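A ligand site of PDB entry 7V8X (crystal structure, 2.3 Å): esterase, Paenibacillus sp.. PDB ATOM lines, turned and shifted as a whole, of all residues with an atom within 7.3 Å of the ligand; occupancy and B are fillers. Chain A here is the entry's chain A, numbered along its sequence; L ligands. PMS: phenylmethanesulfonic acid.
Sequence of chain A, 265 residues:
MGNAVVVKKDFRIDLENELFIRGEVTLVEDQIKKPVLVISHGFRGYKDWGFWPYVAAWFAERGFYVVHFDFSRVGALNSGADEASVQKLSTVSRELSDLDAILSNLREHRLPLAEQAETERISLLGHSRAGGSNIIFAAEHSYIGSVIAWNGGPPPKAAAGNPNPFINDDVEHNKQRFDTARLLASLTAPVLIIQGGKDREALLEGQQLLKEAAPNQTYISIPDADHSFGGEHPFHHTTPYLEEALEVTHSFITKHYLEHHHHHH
NE2 of His 127 lies close to O2S of the ligand, 3.3 Å away.
The side-chain hydroxyl (OG) of Ser 128 is covalently linked to a sulfur (S) of the ligand, at 1.5 Å.
O2S of the ligand sits close to NE2 of His 227 (3.1 Å).
Gly 42 touches the ligand.
Phe 43 touches the ligand (CB to C5, 3.1 Å).
Arg 44 touches the ligand.
Arg 129 touches the ligand (CB to C4, 3.3 Å).
Ser 228 touches the ligand.
Hydrophobic or aromatic side chains that line the ligand: Phe 43, His 127 and His 227.
A ring nitrogen (ND1) of His 227 is in hydrogen-bond range of the side-chain carboxylate (OD2) of Asp 199.
NH2 of Arg 73 sits at hydrogen-bond distance from O of Gly 42, 3.5 Å away.
The side-chain carboxylate (OE1) of Glu 95 is in salt-bridge range of the guanidinium group (NE) of Arg 129.
A ring nitrogen (NE2) of His 227 sits at hydrogen-bond distance from the side-chain hydroxyl (OG) of Ser 128 (2.9 Å).
NE2 of His 127 is in hydrogen-bond range of O of His 227, at 3.3 Å.
The backbone NH (N) of Ser 128 is in hydrogen-bond range of the backbone carbonyl oxygen (O) of Trp 150, 3.0 Å away.
The side-chain amide nitrogen of Asn 151 sits at hydrogen-bond distance from the backbone carbonyl oxygen of His 227 (2.8 Å).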
ATOM      1  N   HIS A  41     -23.722  10.077 -29.952  1.00  0.00           N
ATOM      2  CA  HIS A  41     -24.509  11.067 -29.235  1.00  0.00           C
ATOM      3  C   HIS A  41     -24.101  12.489 -29.652  1.00  0.00           C
ATOM      4  O   HIS A  41     -23.196  12.702 -30.465  1.00  0.00           O
ATOM      5  CB  HIS A  41     -24.382  10.855 -27.724  1.00  0.00           C
ATOM      6  CG  HIS A  41     -22.989  10.943 -27.205  1.00  0.00           C
ATOM      7  ND1 HIS A  41     -22.241  12.102 -27.275  1.00  0.00           N
ATOM      8  CD2 HIS A  41     -22.221  10.045 -26.548  1.00  0.00           C
ATOM      9  CE1 HIS A  41     -21.060  11.902 -26.719  1.00  0.00           C
ATOM     10  NE2 HIS A  41     -21.025  10.661 -26.267  1.00  0.00           N
ATOM     11  N   GLY A  42     -24.692  13.511 -29.034  1.00  0.00           N
ATOM     12  CA  GLY A  42     -24.333  14.917 -29.352  1.00  0.00           C
ATOM     13  C   GLY A  42     -23.147  15.444 -28.568  1.00  0.00           C
ATOM     14  O   GLY A  42     -22.793  14.828 -27.574  1.00  0.00           O
ATOM     15  N   PHE A  43     -22.579  16.596 -28.964  1.00  0.00           N
ATOM     16  CA  PHE A  43     -21.341  17.126 -28.301  1.00  0.00           C
ATOM     17  C   PHE A  43     -21.615  17.651 -26.898  1.00  0.00           C
ATOM     18  O   PHE A  43     -20.657  17.873 -26.130  1.00  0.00           O
ATOM     19  CB  PHE A  43     -20.444  17.930 -29.271  1.00  0.00           C
ATOM     20  CG  PHE A  43     -19.555  19.008 -28.716  1.00  0.00           C
ATOM     21  CD1 PHE A  43     -18.279  18.728 -28.264  1.00  0.00           C
ATOM     22  CD2 PHE A  43     -19.968  20.337 -28.705  1.00  0.00           C
ATOM     23  CE1 PHE A  43     -17.464  19.733 -27.772  1.00  0.00           C
ATOM     24  CE2 PHE A  43     -19.146  21.337 -28.220  1.00  0.00           C
ATOM     25  CZ  PHE A  43     -17.891  21.033 -27.757  1.00  0.00           C
ATOM     26  N   ARG A  44     -22.877  17.803 -26.531  1.00  0.00           N
ATOM     27  CA  ARG A  44     -23.168  18.165 -25.123  1.00  0.00           C
ATOM     28  C   ARG A  44     -23.709  16.903 -24.440  1.00  0.00           C
ATOM     29  O   ARG A  44     -23.839  16.933 -23.207  1.00  0.00           O
ATOM     30  CB  ARG A  44     -24.140  19.337 -25.076  1.00  0.00           C
ATOM     31  CG  ARG A  44     -23.458  20.699 -25.170  1.00  0.00           C
ATOM     32  CD  ARG A  44     -22.272  20.778 -24.231  1.00  0.00           C
ATOM     33  NE  ARG A  44     -21.367  21.870 -24.553  1.00  0.00           N
ATOM     34  CZ  ARG A  44     -20.050  21.751 -24.646  1.00  0.00           C
ATOM     35  NH1 ARG A  44     -19.478  20.573 -24.429  1.00  0.00           N
ATOM     36  NH2 ARG A  44     -19.308  22.797 -24.936  1.00  0.00           N
ATOM     37  N   GLY A  45     -23.939  15.832 -25.207  1.00  0.00           N
ATOM     38  CA  GLY A  45     -24.568  14.625 -24.635  1.00  0.00           C
ATOM     39  C   GLY A  45     -23.621  13.521 -24.247  1.00  0.00           C
ATOM     40  O   GLY A  45     -22.402  13.754 -24.284  1.00  0.00           O
ATOM     41  N   TRP A  49     -27.410   9.793 -21.251  1.00  0.00           N
ATOM     42  CA  TRP A  49     -28.215  11.026 -21.179  1.00  0.00           C
ATOM     43  C   TRP A  49     -29.540  10.862 -21.862  1.00  0.00           C
ATOM     44  O   TRP A  49     -29.562  10.261 -22.960  1.00  0.00           O
ATOM     45  CB  TRP A  49     -27.472  12.177 -21.865  1.00  0.00           C
ATOM     46  CG  TRP A  49     -28.287  13.404 -22.129  1.00  0.00           C
ATOM     47  CD1 TRP A  49     -29.024  13.669 -23.241  1.00  0.00           C
ATOM     48  CD2 TRP A  49     -28.469  14.537 -21.248  1.00  0.00           C
ATOM     49  NE1 TRP A  49     -29.648  14.888 -23.128  1.00  0.00           N
ATOM     50  CE2 TRP A  49     -29.327  15.441 -21.925  1.00  0.00           C
ATOM     51  CE3 TRP A  49     -27.999  14.883 -19.981  1.00  0.00           C
ATOM     52  CZ2 TRP A  49     -29.701  16.661 -21.361  1.00  0.00           C
ATOM     53  CZ3 TRP A  49     -28.365  16.087 -19.431  1.00  0.00           C
ATOM     54  CH2 TRP A  49     -29.213  16.959 -20.107  1.00  0.00           C
ATOM     55  N   PHE A  51     -32.633  10.347 -23.908  1.00  0.00           N
ATOM     56  CA  PHE A  51     -33.368   9.330 -24.638  1.00  0.00           C
ATOM     57  C   PHE A  51     -32.477   8.236 -25.244  1.00  0.00           C
ATOM     58  O   PHE A  51     -33.000   7.313 -25.890  1.00  0.00           O
ATOM     59  CB  PHE A  51     -34.256   9.978 -25.722  1.00  0.00           C
ATOM     60  CG  PHE A  51     -33.524  10.869 -26.712  1.00  0.00           C
ATOM     61  CD1 PHE A  51     -32.429  10.404 -27.437  1.00  0.00           C
ATOM     62  CD2 PHE A  51     -33.972  12.147 -26.958  1.00  0.00           C
ATOM     63  CE1 PHE A  51     -31.777  11.220 -28.370  1.00  0.00           C
ATOM     64  CE2 PHE A  51     -33.327  12.955 -27.879  1.00  0.00           C
ATOM     65  CZ  PHE A  51     -32.229  12.498 -28.588  1.00  0.00           C
ATOM     66  N   TRP A  52     -31.162   8.301 -25.045  1.00  0.00           N
ATOM     67  CA  TRP A  52     -30.299   7.306 -25.679  1.00  0.00           C
ATOM     68  C   TRP A  52     -30.580   5.891 -25.179  1.00  0.00           C
ATOM     69  O   TRP A  52     -30.759   4.993 -26.018  1.00  0.00           O
ATOM     70  CB  TRP A  52     -28.832   7.718 -25.538  1.00  0.00           C
ATOM     71  CG  TRP A  52     -28.487   8.828 -26.505  1.00  0.00           C
ATOM     72  CD1 TRP A  52     -27.725   9.929 -26.239  1.00  0.00           C
ATOM     73  CD2 TRP A  52     -28.913   8.938 -27.870  1.00  0.00           C
ATOM     74  NE1 TRP A  52     -27.646  10.721 -27.363  1.00  0.00           N
ATOM     75  CE2 TRP A  52     -28.352  10.123 -28.374  1.00  0.00           C
ATOM     76  CE3 TRP A  52     -29.676   8.148 -28.725  1.00  0.00           C
ATOM     77  CZ2 TRP A  52     -28.556  10.537 -29.682  1.00  0.00           C
ATOM     78  CZ3 TRP A  52     -29.879   8.561 -30.033  1.00  0.00           C
ATOM     79  CH2 TRP A  52     -29.332   9.749 -30.489  1.00  0.00           C
ATOM     80  N   ARG A  73     -13.781  11.911 -25.560  1.00  0.00           N
ATOM     81  CA  ARG A  73     -13.704  13.157 -24.795  1.00  0.00           C
ATOM     82  C   ARG A  73     -14.590  13.094 -23.552  1.00  0.00           C
ATOM     83  O   ARG A  73     -14.258  13.703 -22.531  1.00  0.00           O
ATOM     84  CB  ARG A  73     -14.110  14.347 -25.681  1.00  0.00           C
ATOM     85  CG  ARG A  73     -15.586  14.534 -25.766  1.00  0.00           C
ATOM     86  CD  ARG A  73     -16.002  14.987 -27.131  1.00  0.00           C
ATOM     87  NE  ARG A  73     -17.447  14.910 -27.285  1.00  0.00           N
ATOM     88  CZ  ARG A  73     -18.089  14.964 -28.449  1.00  0.00           C
ATOM     89  NH1 ARG A  73     -17.438  15.086 -29.594  1.00  0.00           N
ATOM     90  NH2 ARG A  73     -19.421  14.871 -28.459  1.00  0.00           N
ATOM     91  N   GLU A  95     -13.829  12.706 -33.537  1.00  0.00           N
ATOM     92  CA  GLU A  95     -15.053  11.919 -33.615  1.00  0.00           C
ATOM     93  C   GLU A  95     -14.950  10.861 -34.705  1.00  0.00           C
ATOM     94  O   GLU A  95     -15.352   9.713 -34.484  1.00  0.00           O
ATOM     95  CB  GLU A  95     -16.260  12.842 -33.848  1.00  0.00           C
ATOM     96  CG  GLU A  95     -16.499  13.843 -32.722  1.00  0.00           C
ATOM     97  CD  GLU A  95     -17.785  14.638 -32.878  1.00  0.00           C
ATOM     98  OE1 GLU A  95     -17.805  15.813 -32.422  1.00  0.00           O
ATOM     99  OE2 GLU A  95     -18.762  14.108 -33.489  1.00  0.00           O
ATOM    100  N   HIS A 127     -26.499  12.648 -33.775  1.00  0.00           N
ATOM    101  CA  HIS A 127     -27.240  13.742 -33.154  1.00  0.00           C
ATOM    102  C   HIS A 127     -26.390  14.995 -33.178  1.00  0.00           C
ATOM    103  O   HIS A 127     -25.226  14.965 -32.761  1.00  0.00           O
ATOM    104  CB  HIS A 127     -27.653  13.391 -31.726  1.00  0.00           C
ATOM    105  CG  HIS A 127     -28.731  14.278 -31.155  1.00  0.00           C
ATOM    106  ND1 HIS A 127     -28.951  14.408 -29.795  1.00  0.00           N
ATOM    107  CD2 HIS A 127     -29.632  15.091 -31.755  1.00  0.00           C
ATOM    108  CE1 HIS A 127     -29.943  15.247 -29.592  1.00  0.00           C
ATOM    109  NE2 HIS A 127     -30.376  15.684 -30.760  1.00  0.00           N
ATOM    110  N   SER A 128     -26.936  16.057 -33.767  1.00  0.00           N
ATOM    111  CA  SER A 128     -26.574  17.469 -33.612  1.00  0.00           C
ATOM    112  C   SER A 128     -25.298  17.883 -34.335  1.00  0.00           C
ATOM    113  O   SER A 128     -25.316  18.835 -35.124  1.00  0.00           O
ATOM    114  CB  SER A 128     -26.452  17.827 -32.116  1.00  0.00           C
ATOM    115  OG  SER A 128     -27.658  17.843 -31.353  1.00  0.00           O
ATOM    116  N   ARG A 129     -24.190  17.195 -34.100  1.00  0.00           N
ATOM    117  CA  ARG A 129     -22.977  17.473 -34.851  1.00  0.00           C
ATOM    118  C   ARG A 129     -22.325  16.158 -35.221  1.00  0.00           C
ATOM    119  O   ARG A 129     -21.534  16.035 -36.162  1.00  0.00           O
ATOM    120  CB  ARG A 129     -22.102  18.349 -33.949  1.00  0.00           C
ATOM    121  CG  ARG A 129     -20.601  18.366 -34.282  1.00  0.00           C
ATOM    122  CD  ARG A 129     -19.843  18.394 -32.970  1.00  0.00           C
ATOM    123  NE  ARG A 129     -18.430  18.051 -33.044  1.00  0.00           N
ATOM    124  CZ  ARG A 129     -17.444  18.931 -32.911  1.00  0.00           C
ATOM    125  NH1 ARG A 129     -17.682  20.227 -32.790  1.00  0.00           N
ATOM    126  NH2 ARG A 129     -16.195  18.494 -32.876  1.00  0.00           N
ATOM    127  N   ALA A 130     -22.671  15.148 -34.429  1.00  0.00           N
ATOM    128  CA  ALA A 130     -22.456  13.787 -34.850  1.00  0.00           C
ATOM    129  C   ALA A 130     -23.253  13.480 -36.106  1.00  0.00           C
ATOM    130  O   ALA A 130     -22.848  12.603 -36.867  1.00  0.00           O
ATOM    131  CB  ALA A 130     -22.802  12.805 -33.728  1.00  0.00           C
ATOM    132  N   TRP A 150     -30.089  13.497 -36.849  1.00  0.00           N
ATOM    133  CA  TRP A 150     -31.153  14.148 -36.099  1.00  0.00           C
ATOM    134  C   TRP A 150     -30.650  15.541 -35.753  1.00  0.00           C
ATOM    135  O   TRP A 150     -29.666  15.686 -35.019  1.00  0.00           O
ATOM    136  CB  TRP A 150     -31.495  13.345 -34.849  1.00  0.00           C
ATOM    137  CG  TRP A 150     -32.338  12.140 -35.101  1.00  0.00           C
ATOM    138  CD1 TRP A 150     -32.814  11.700 -36.302  1.00  0.00           C
ATOM    139  CD2 TRP A 150     -32.815  11.223 -34.111  1.00  0.00           C
ATOM    140  NE1 TRP A 150     -33.573  10.545 -36.119  1.00  0.00           N
ATOM    141  CE2 TRP A 150     -33.574  10.229 -34.787  1.00  0.00           C
ATOM    142  CE3 TRP A 150     -32.668  11.126 -32.713  1.00  0.00           C
ATOM    143  CZ2 TRP A 150     -34.187   9.169 -34.100  1.00  0.00           C
ATOM    144  CZ3 TRP A 150     -33.266  10.070 -32.045  1.00  0.00           C
ATOM    145  CH2 TRP A 150     -34.017   9.109 -32.733  1.00  0.00           C
ATOM    146  N   ASN A 151     -31.296  16.564 -36.344  1.00  0.00           N
ATOM    147  CA  ASN A 151     -31.004  17.973 -36.070  1.00  0.00           C
ATOM    148  C   ASN A 151     -29.515  18.261 -36.223  1.00  0.00           C
ATOM    149  O   ASN A 151     -28.893  18.921 -35.387  1.00  0.00           O
ATOM    150  CB  ASN A 151     -31.519  18.390 -34.678  1.00  0.00           C
ATOM    151  CG  ASN A 151     -33.019  18.213 -34.543  1.00  0.00           C
ATOM    152  OD1 ASN A 151     -33.780  18.601 -35.425  1.00  0.00           O
ATOM    153  ND2 ASN A 151     -33.454  17.554 -33.466  1.00  0.00           N
ATOM    154  N   ASP A 199     -36.070  25.205 -33.965  1.00  0.00           N
ATOM    155  CA  ASP A 199     -34.653  25.103 -33.649  1.00  0.00           C
ATOM    156  C   ASP A 199     -33.953  26.340 -34.181  1.00  0.00           C
ATOM    157  O   ASP A 199     -34.499  27.108 -34.982  1.00  0.00           O
ATOM    158  CB  ASP A 199     -34.023  23.821 -34.221  1.00  0.00           C
ATOM    159  CG  ASP A 199     -32.741  23.419 -33.479  1.00  0.00           C
ATOM    160  OD1 ASP A 199     -32.114  24.279 -32.842  1.00  0.00           O
ATOM    161  OD2 ASP A 199     -32.363  22.224 -33.534  1.00  0.00           O
ATOM    162  N   LEU A 203     -29.158  26.890 -38.058  1.00  0.00           N
ATOM    163  CA  LEU A 203     -29.222  25.481 -38.456  1.00  0.00           C
ATOM    164  C   LEU A 203     -30.302  25.253 -39.507  1.00  0.00           C
ATOM    165  O   LEU A 203     -30.106  24.452 -40.424  1.00  0.00           O
ATOM    166  CB  LEU A 203     -29.416  24.586 -37.231  1.00  0.00           C
ATOM    167  CG  LEU A 203     -29.782  23.105 -37.411  1.00  0.00           C
ATOM    168  CD1 LEU A 203     -28.644  22.339 -38.090  1.00  0.00           C
ATOM    169  CD2 LEU A 203     -30.115  22.433 -36.075  1.00  0.00           C
ATOM    170  N   HIS A 227     -34.500  21.140 -30.437  1.00  0.00           N
ATOM    171  CA  HIS A 227     -33.267  20.505 -30.862  1.00  0.00           C
ATOM    172  C   HIS A 227     -33.159  19.069 -30.385  1.00  0.00           C
ATOM    173  O   HIS A 227     -32.392  18.299 -30.961  1.00  0.00           O
ATOM    174  CB  HIS A 227     -32.078  21.321 -30.366  1.00  0.00           C
ATOM    175  CG  HIS A 227     -30.781  20.989 -31.057  1.00  0.00           C
ATOM    176  ND1 HIS A 227     -30.668  20.904 -32.430  1.00  0.00           N
ATOM    177  CD2 HIS A 227     -29.531  20.811 -30.568  1.00  0.00           C
ATOM    178  CE1 HIS A 227     -29.411  20.635 -32.745  1.00  0.00           C
ATOM    179  NE2 HIS A 227     -28.702  20.579 -31.637  1.00  0.00           N
ATOM    180  N   SER A 228     -33.951  18.682 -29.377  1.00  0.00           N
ATOM    181  CA  SER A 228     -33.832  17.348 -28.795  1.00  0.00           C
ATOM    182  C   SER A 228     -35.139  16.577 -28.827  1.00  0.00           C
ATOM    183  O   SER A 228     -35.268  15.582 -28.118  1.00  0.00           O
ATOM    184  CB  SER A 228     -33.317  17.438 -27.366  1.00  0.00           C
ATOM    185  OG  SER A 228     -32.059  18.096 -27.346  1.00  0.00           O
HETATM  186  C   PMS L   1     -26.536  19.877 -29.420  1.00  0.00           C
HETATM  187  S   PMS L   1     -27.359  18.354 -30.003  1.00  0.00           S
HETATM  188  C1  PMS L   1     -25.211  20.070 -30.158  1.00  0.00           C
HETATM  189  C2  PMS L   1     -25.144  20.870 -31.284  1.00  0.00           C
HETATM  190  C3  PMS L   1     -23.933  21.009 -31.933  1.00  0.00           C
HETATM  191  C4  PMS L   1     -22.802  20.355 -31.444  1.00  0.00           C
HETATM  192  C5  PMS L   1     -22.858  19.546 -30.317  1.00  0.00           C
HETATM  193  C6  PMS L   1     -24.083  19.421 -29.691  1.00  0.00           C
HETATM  194  O2S PMS L   1     -28.785  18.259 -29.512  1.00  0.00           O
HETATM  195  O1S PMS L   1     -26.785  17.163 -29.272  1.00  0.00           O
